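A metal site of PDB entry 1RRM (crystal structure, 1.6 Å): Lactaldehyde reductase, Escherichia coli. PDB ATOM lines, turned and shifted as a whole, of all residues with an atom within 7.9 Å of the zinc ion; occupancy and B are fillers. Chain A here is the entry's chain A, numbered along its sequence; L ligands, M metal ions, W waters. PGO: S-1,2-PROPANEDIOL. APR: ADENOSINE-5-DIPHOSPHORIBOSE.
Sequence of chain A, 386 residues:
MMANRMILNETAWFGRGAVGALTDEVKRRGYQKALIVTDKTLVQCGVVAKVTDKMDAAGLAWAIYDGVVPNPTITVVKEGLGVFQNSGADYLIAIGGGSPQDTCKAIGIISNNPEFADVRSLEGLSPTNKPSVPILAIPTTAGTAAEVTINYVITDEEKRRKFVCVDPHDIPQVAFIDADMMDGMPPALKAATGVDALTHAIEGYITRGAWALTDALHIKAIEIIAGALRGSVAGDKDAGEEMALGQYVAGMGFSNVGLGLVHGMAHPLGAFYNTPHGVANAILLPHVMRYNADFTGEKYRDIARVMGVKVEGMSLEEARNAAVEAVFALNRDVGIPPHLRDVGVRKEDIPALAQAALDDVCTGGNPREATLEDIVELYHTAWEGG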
ATOM      1  N   GLY A 143     -14.659   6.497 -31.297  1.00  0.00           N
ATOM      2  CA  GLY A 143     -14.557   7.191 -30.034  1.00  0.00           C
ATOM      3  C   GLY A 143     -15.130   8.596 -29.833  1.00  0.00           C
ATOM      4  O   GLY A 143     -15.703   8.810 -28.783  1.00  0.00           O
ATOM      5  N   THR A 144     -15.005   9.540 -30.777  1.00  0.00           N
ATOM      6  CA  THR A 144     -15.492  10.896 -30.477  1.00  0.00           C
ATOM      7  C   THR A 144     -16.954  11.243 -30.693  1.00  0.00           C
ATOM      8  O   THR A 144     -17.470  12.173 -30.057  1.00  0.00           O
ATOM      9  CB  THR A 144     -14.681  12.032 -31.190  1.00  0.00           C
ATOM     10  OG1 THR A 144     -15.150  12.190 -32.537  1.00  0.00           O
ATOM     11  CG2 THR A 144     -13.202  11.705 -31.197  1.00  0.00           C
ATOM     12  N   ALA A 145     -17.629  10.517 -31.587  1.00  0.00           N
ATOM     13  CA  ALA A 145     -19.030  10.772 -31.906  1.00  0.00           C
ATOM     14  C   ALA A 145     -19.220  12.185 -32.472  1.00  0.00           C
ATOM     15  O   ALA A 145     -20.310  12.733 -32.409  1.00  0.00           O
ATOM     16  CB  ALA A 145     -19.918  10.592 -30.669  1.00  0.00           C
ATOM     17  N   VAL A 153     -13.956  21.020 -30.746  1.00  0.00           N
ATOM     18  CA  VAL A 153     -12.905  21.667 -29.973  1.00  0.00           C
ATOM     19  C   VAL A 153     -11.696  22.031 -30.813  1.00  0.00           C
ATOM     20  O   VAL A 153     -11.119  21.193 -31.502  1.00  0.00           O
ATOM     21  CB  VAL A 153     -12.487  20.774 -28.795  1.00  0.00           C
ATOM     22  CG1 VAL A 153     -12.018  19.425 -29.304  1.00  0.00           C
ATOM     23  CG2 VAL A 153     -11.397  21.455 -27.975  1.00  0.00           C
ATOM     24  N   THR A 193      -9.278   5.687 -28.526  1.00  0.00           N
ATOM     25  CA  THR A 193     -10.560   6.257 -28.938  1.00  0.00           C
ATOM     26  C   THR A 193     -11.730   5.525 -28.289  1.00  0.00           C
ATOM     27  O   THR A 193     -12.778   6.126 -28.031  1.00  0.00           O
ATOM     28  CB  THR A 193     -10.727   6.276 -30.491  1.00  0.00           C
ATOM     29  OG1 THR A 193     -10.721   4.944 -31.023  1.00  0.00           O
ATOM     30  CG2 THR A 193      -9.613   7.084 -31.135  1.00  0.00           C
ATOM     31  N   VAL A 195     -11.721   4.228 -25.214  1.00  0.00           N
ATOM     32  CA  VAL A 195     -11.898   4.668 -23.843  1.00  0.00           C
ATOM     33  C   VAL A 195     -12.430   6.106 -23.834  1.00  0.00           C
ATOM     34  O   VAL A 195     -13.077   6.520 -22.889  1.00  0.00           O
ATOM     35  CB  VAL A 195     -10.600   4.581 -23.033  1.00  0.00           C
ATOM     36  CG1 VAL A 195     -10.807   5.160 -21.639  1.00  0.00           C
ATOM     37  CG2 VAL A 195     -10.171   3.121 -22.925  1.00  0.00           C
ATOM     38  N   ASP A 196     -12.149   6.854 -24.899  1.00  0.00           N
ATOM     39  CA  ASP A 196     -12.670   8.217 -25.007  1.00  0.00           C
ATOM     40  C   ASP A 196     -14.193   8.056 -25.061  1.00  0.00           C
ATOM     41  O   ASP A 196     -14.930   8.752 -24.362  1.00  0.00           O
ATOM     42  CB  ASP A 196     -12.148   8.881 -26.289  1.00  0.00           C
ATOM     43  CG  ASP A 196     -12.765  10.249 -26.554  1.00  0.00           C
ATOM     44  OD1 ASP A 196     -13.086  10.978 -25.591  1.00  0.00           O
ATOM     45  OD2 ASP A 196     -12.931  10.618 -27.736  1.00  0.00           O
ATOM     46  N   ALA A 197     -14.655   7.117 -25.882  1.00  0.00           N
ATOM     47  CA  ALA A 197     -16.083   6.848 -26.009  1.00  0.00           C
ATOM     48  C   ALA A 197     -16.682   6.383 -24.679  1.00  0.00           C
ATOM     49  O   ALA A 197     -17.772   6.806 -24.304  1.00  0.00           O
ATOM     50  CB  ALA A 197     -16.330   5.791 -27.089  1.00  0.00           C
ATOM     51  N   THR A 199     -15.605   7.101 -21.777  1.00  0.00           N
ATOM     52  CA  THR A 199     -15.600   8.280 -20.913  1.00  0.00           C
ATOM     53  C   THR A 199     -16.826   9.140 -21.230  1.00  0.00           C
ATOM     54  O   THR A 199     -17.478   9.672 -20.337  1.00  0.00           O
ATOM     55  CB  THR A 199     -14.324   9.133 -21.118  1.00  0.00           C
ATOM     56  OG1 THR A 199     -13.174   8.381 -20.735  1.00  0.00           O
ATOM     57  CG2 THR A 199     -14.387  10.397 -20.277  1.00  0.00           C
ATOM     58  N   HIS A 200     -17.141   9.262 -22.517  1.00  0.00           N
ATOM     59  CA  HIS A 200     -18.306  10.031 -22.938  1.00  0.00           C
ATOM     60  C   HIS A 200     -19.574   9.462 -22.296  1.00  0.00           C
ATOM     61  O   HIS A 200     -20.396  10.204 -21.750  1.00  0.00           O
ATOM     62  CB  HIS A 200     -18.457   9.972 -24.459  1.00  0.00           C
ATOM     63  CG  HIS A 200     -17.437  10.769 -25.205  1.00  0.00           C
ATOM     64  ND1 HIS A 200     -17.174  10.578 -26.544  1.00  0.00           N
ATOM     65  CD2 HIS A 200     -16.615  11.772 -24.800  1.00  0.00           C
ATOM     66  CE1 HIS A 200     -16.242  11.427 -26.936  1.00  0.00           C
ATOM     67  NE2 HIS A 200     -15.882  12.159 -25.886  1.00  0.00           N
ATOM     68  N   GLU A 203     -19.323   9.800 -18.217  1.00  0.00           N
ATOM     69  CA  GLU A 203     -19.513  11.184 -17.789  1.00  0.00           C
ATOM     70  C   GLU A 203     -20.934  11.639 -18.106  1.00  0.00           C
ATOM     71  O   GLU A 203     -21.592  12.287 -17.294  1.00  0.00           O
ATOM     72  CB  GLU A 203     -18.519  12.133 -18.473  1.00  0.00           C
ATOM     73  CG  GLU A 203     -17.065  11.948 -18.040  1.00  0.00           C
ATOM     74  CD  GLU A 203     -16.322  13.267 -18.007  1.00  0.00           C
ATOM     75  OE1 GLU A 203     -16.213  13.874 -16.901  1.00  0.00           O
ATOM     76  OE2 GLU A 203     -15.845  13.707 -19.081  1.00  0.00           O
ATOM     77  N   PHE A 254     -24.511  12.401 -24.495  1.00  0.00           N
ATOM     78  CA  PHE A 254     -23.713  13.480 -23.925  1.00  0.00           C
ATOM     79  C   PHE A 254     -23.739  14.816 -24.658  1.00  0.00           C
ATOM     80  O   PHE A 254     -23.582  15.873 -24.049  1.00  0.00           O
ATOM     81  CB  PHE A 254     -22.279  13.014 -23.656  1.00  0.00           C
ATOM     82  CG  PHE A 254     -21.337  13.172 -24.817  1.00  0.00           C
ATOM     83  CD1 PHE A 254     -20.684  14.381 -25.052  1.00  0.00           C
ATOM     84  CD2 PHE A 254     -21.063  12.084 -25.647  1.00  0.00           C
ATOM     85  CE1 PHE A 254     -19.764  14.503 -26.082  1.00  0.00           C
ATOM     86  CE2 PHE A 254     -20.138  12.207 -26.690  1.00  0.00           C
ATOM     87  CZ  PHE A 254     -19.486  13.407 -26.902  1.00  0.00           C
ATOM     88  N   LEU A 259     -20.768  16.586 -20.117  1.00  0.00           N
ATOM     89  CA  LEU A 259     -19.794  15.628 -19.606  1.00  0.00           C
ATOM     90  C   LEU A 259     -19.388  15.991 -18.189  1.00  0.00           C
ATOM     91  O   LEU A 259     -20.236  16.176 -17.319  1.00  0.00           O
ATOM     92  CB  LEU A 259     -18.574  15.587 -20.526  1.00  0.00           C
ATOM     93  CG  LEU A 259     -18.907  15.079 -21.939  1.00  0.00           C
ATOM     94  CD1 LEU A 259     -17.745  15.344 -22.882  1.00  0.00           C
ATOM     95  CD2 LEU A 259     -19.237  13.593 -21.873  1.00  0.00           C
ATOM     96  N   HIS A 263     -13.168  15.249 -18.956  1.00  0.00           N
ATOM     97  CA  HIS A 263     -12.884  16.010 -20.174  1.00  0.00           C
ATOM     98  C   HIS A 263     -12.337  17.391 -19.843  1.00  0.00           C
ATOM     99  O   HIS A 263     -11.486  17.906 -20.564  1.00  0.00           O
ATOM    100  CB  HIS A 263     -14.138  16.117 -21.036  1.00  0.00           C
ATOM    101  CG  HIS A 263     -14.309  14.972 -21.987  1.00  0.00           C
ATOM    102  ND1 HIS A 263     -14.530  13.683 -21.571  1.00  0.00           N
ATOM    103  CD2 HIS A 263     -14.199  14.920 -23.342  1.00  0.00           C
ATOM    104  CE1 HIS A 263     -14.551  12.874 -22.619  1.00  0.00           C
ATOM    105  NE2 HIS A 263     -14.353  13.605 -23.704  1.00  0.00           N
ATOM    106  N   ALA A 266      -8.804  16.760 -19.224  1.00  0.00           N
ATOM    107  CA  ALA A 266      -8.128  16.197 -20.384  1.00  0.00           C
ATOM    108  C   ALA A 266      -7.778  17.272 -21.427  1.00  0.00           C
ATOM    109  O   ALA A 266      -6.728  17.203 -22.073  1.00  0.00           O
ATOM    110  CB  ALA A 266      -8.992  15.119 -21.014  1.00  0.00           C
ATOM    111  N   HIS A 267      -8.649  18.256 -21.593  1.00  0.00           N
ATOM    112  CA  HIS A 267      -8.414  19.296 -22.577  1.00  0.00           C
ATOM    113  C   HIS A 267      -7.131  20.089 -22.392  1.00  0.00           C
ATOM    114  O   HIS A 267      -6.392  20.313 -23.348  1.00  0.00           O
ATOM    115  CB  HIS A 267      -9.634  20.219 -22.654  1.00  0.00           C
ATOM    116  CG  HIS A 267     -10.807  19.598 -23.349  1.00  0.00           C
ATOM    117  ND1 HIS A 267     -12.086  20.075 -23.227  1.00  0.00           N
ATOM    118  CD2 HIS A 267     -10.877  18.526 -24.174  1.00  0.00           C
ATOM    119  CE1 HIS A 267     -12.909  19.327 -23.953  1.00  0.00           C
ATOM    120  NE2 HIS A 267     -12.199  18.383 -24.536  1.00  0.00           N
ATOM    121  N   HIS A 277      -6.287  12.856 -26.978  1.00  0.00           N
ATOM    122  CA  HIS A 277      -7.492  13.012 -26.170  1.00  0.00           C
ATOM    123  C   HIS A 277      -7.902  11.747 -25.412  1.00  0.00           C
ATOM    124  O   HIS A 277      -8.129  11.784 -24.193  1.00  0.00           O
ATOM    125  CB  HIS A 277      -8.630  13.477 -27.073  1.00  0.00           C
ATOM    126  CG  HIS A 277      -9.907  13.785 -26.346  1.00  0.00           C
ATOM    127  ND1 HIS A 277     -10.004  14.780 -25.406  1.00  0.00           N
ATOM    128  CD2 HIS A 277     -11.145  13.260 -26.462  1.00  0.00           C
ATOM    129  CE1 HIS A 277     -11.248  14.865 -24.976  1.00  0.00           C
ATOM    130  NE2 HIS A 277     -11.968  13.948 -25.600  1.00  0.00           N
ATOM    131  N   GLY A 278      -8.010  10.629 -26.121  1.00  0.00           N
ATOM    132  CA  GLY A 278      -8.406   9.389 -25.489  1.00  0.00           C
ATOM    133  C   GLY A 278      -7.474   8.879 -24.404  1.00  0.00           C
ATOM    134  O   GLY A 278      -7.932   8.295 -23.411  1.00  0.00           O
ATOM    135  N   ASN A 281      -8.072  11.095 -21.272  1.00  0.00           N
ATOM    136  CA  ASN A 281      -9.308  10.690 -20.612  1.00  0.00           C
ATOM    137  C   ASN A 281      -9.135   9.365 -19.885  1.00  0.00           C
ATOM    138  O   ASN A 281      -9.554   9.213 -18.737  1.00  0.00           O
ATOM    139  CB  ASN A 281     -10.459  10.546 -21.623  1.00  0.00           C
ATOM    140  CG  ASN A 281     -10.972  11.879 -22.120  1.00  0.00           C
ATOM    141  OD1 ASN A 281     -11.064  12.846 -21.363  1.00  0.00           O
ATOM    142  ND2 ASN A 281     -11.341  11.928 -23.390  1.00  0.00           N
ATOM    143  N   CYS A 362     -16.632  21.898 -20.339  1.00  0.00           N
ATOM    144  CA  CYS A 362     -17.185  20.639 -19.859  1.00  0.00           C
ATOM    145  C   CYS A 362     -17.195  20.446 -18.341  1.00  0.00           C
ATOM    146  O   CYS A 362     -18.035  19.710 -17.811  1.00  0.00           O
ATOM    147  CB  CYS A 362     -16.421  19.466 -20.498  1.00  0.00           C
ATOM    148  SG  CYS A 362     -16.388  19.496 -22.303  1.00  0.00           S
HETATM  149  C1  PGO L   1     -16.083  15.392 -26.764  1.00  0.00           C
HETATM  150  C2  PGO L   1     -16.697  16.854 -26.768  1.00  0.00           C
HETATM  151  C3  PGO L   1     -17.709  16.814 -27.907  1.00  0.00           C
HETATM  152  O1  PGO L   1     -14.709  15.201 -26.343  1.00  0.00           O
HETATM  153  O2  PGO L   1     -15.561  17.638 -26.955  1.00  0.00           O
HETATM  154  N1  APR L   2      -6.657   4.374 -39.502  1.00  0.00           N
HETATM  155  C2  APR L   2      -5.399   4.901 -39.199  1.00  0.00           C
HETATM  156  N3  APR L   2      -5.142   6.043 -38.626  1.00  0.00           N
HETATM  157  C4  APR L   2      -6.284   6.750 -38.318  1.00  0.00           C
HETATM  158  C5  APR L   2      -7.596   6.384 -38.548  1.00  0.00           C
HETATM  159  C6  APR L   2      -7.797   5.112 -39.186  1.00  0.00           C
HETATM  160  N6  APR L   2      -8.986   4.601 -39.475  1.00  0.00           N
HETATM  161  N7  APR L   2      -8.472   7.358 -38.107  1.00  0.00           N
HETATM  162  C8  APR L   2      -7.683   8.314 -37.600  1.00  0.00           C
HETATM  163  N9  APR L   2      -6.344   8.002 -37.715  1.00  0.00           N
HETATM  164  C1' APR L   2      -5.151   8.730 -37.306  1.00  0.00           C
HETATM  165  C2' APR L   2      -5.115  10.163 -37.790  1.00  0.00           C
HETATM  166  O2' APR L   2      -4.659  10.296 -39.145  1.00  0.00           O
HETATM  167  C3' APR L   2      -4.180  10.853 -36.791  1.00  0.00           C
HETATM  168  O3' APR L   2      -2.767  10.759 -37.071  1.00  0.00           O
HETATM  169  O4' APR L   2      -5.116   8.845 -35.906  1.00  0.00           O
HETATM  170  C4' APR L   2      -4.531  10.112 -35.494  1.00  0.00           C
HETATM  171  C5' APR L   2      -5.479  10.817 -34.540  1.00  0.00           C
HETATM  172  O5' APR L   2      -6.710  11.217 -35.197  1.00  0.00           O
HETATM  173  PA  APR L   2      -7.693  12.250 -34.449  1.00  0.00           P
HETATM  174  O1A APR L   2      -8.781  12.668 -35.368  1.00  0.00           O
HETATM  175  O2A APR L   2      -6.957  13.440 -33.993  1.00  0.00           O
HETATM  176  O3A APR L   2      -8.203  11.393 -33.242  1.00  0.00           O
HETATM  177  PB  APR L   2      -9.691  11.233 -32.534  1.00  0.00           P
HETATM  178  O1B APR L   2      -9.557  10.485 -31.266  1.00  0.00           O
HETATM  179  O2B APR L   2     -10.556  10.530 -33.495  1.00  0.00           O
HETATM  180  O5D APR L   2     -10.131  12.728 -32.339  1.00  0.00           O
HETATM  181  C5D APR L   2      -9.437  13.508 -31.392  1.00  0.00           C
HETATM  182  O4D APR L   2     -11.426  14.895 -31.150  1.00  0.00           O
HETATM  183  O1D APR L   2     -12.876  15.207 -29.341  1.00  0.00           O
HETATM  184  C1D APR L   2     -11.724  15.742 -30.086  1.00  0.00           C
HETATM  185  O2D APR L   2     -10.312  16.942 -28.421  1.00  0.00           O
HETATM  186  C2D APR L   2     -10.460  15.784 -29.262  1.00  0.00           C
HETATM  187  O3D APR L   2      -9.017  17.122 -30.800  1.00  0.00           O
HETATM  188  C3D APR L   2      -9.371  15.806 -30.340  1.00  0.00           C
HETATM  189  C4D APR L   2      -9.997  14.895 -31.379  1.00  0.00           C
HETATM  190 ZN    ZN M   1     -13.962  13.144 -25.784  1.00  0.00          ZN
HETATM  191  O   HOH W   1     -13.859  13.017 -28.003  1.00  0.00           O
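OE2 of Glu 203 is in hydrogen-bond range of ND1 of His 263 (2.8 Å).
NE2 of His 263 lies close to ND2 of Asn 281 (3.5 Å).
The side-chain amide nitrogen (ND2) of Asn 281 lies within hydrogen-bond range of the backbone carbonyl oxygen (O) of His 277, 3.3 Å away.
OD1 of Asp 196 sits close to ND2 of Asn 281, 3.0 Å away.
The backbone carbonyl oxygen of His 263 lies close to a ring nitrogen (ND1) of His 267.
A ring nitrogen (ND1) of His 200 lies within hydrogen-bond range of the backbone carbonyl oxygen of Gly 143.
ND2 of Asn 281 touches the zinc ion (3.8 Å).
Of the 20 residues printed, 5 come within 4 Å of the zinc ion.
The nearest printed residue that does not touch the zinc ion is Leu 259 (5.3 Å).
The zinc ion is bound by NE2 of His 277, NE2 of His 200, NE2 of His 263, water W1, O1 of PGO L1 and OD1 of Asp 196.
The zinc ion has six donor atoms within binding distance.
Water W1 bridges the side-chain carboxylate (OD2) of Asp 196 (2.6 Å) and an oxygen (O1D) of APR L2 (2.7 Å).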
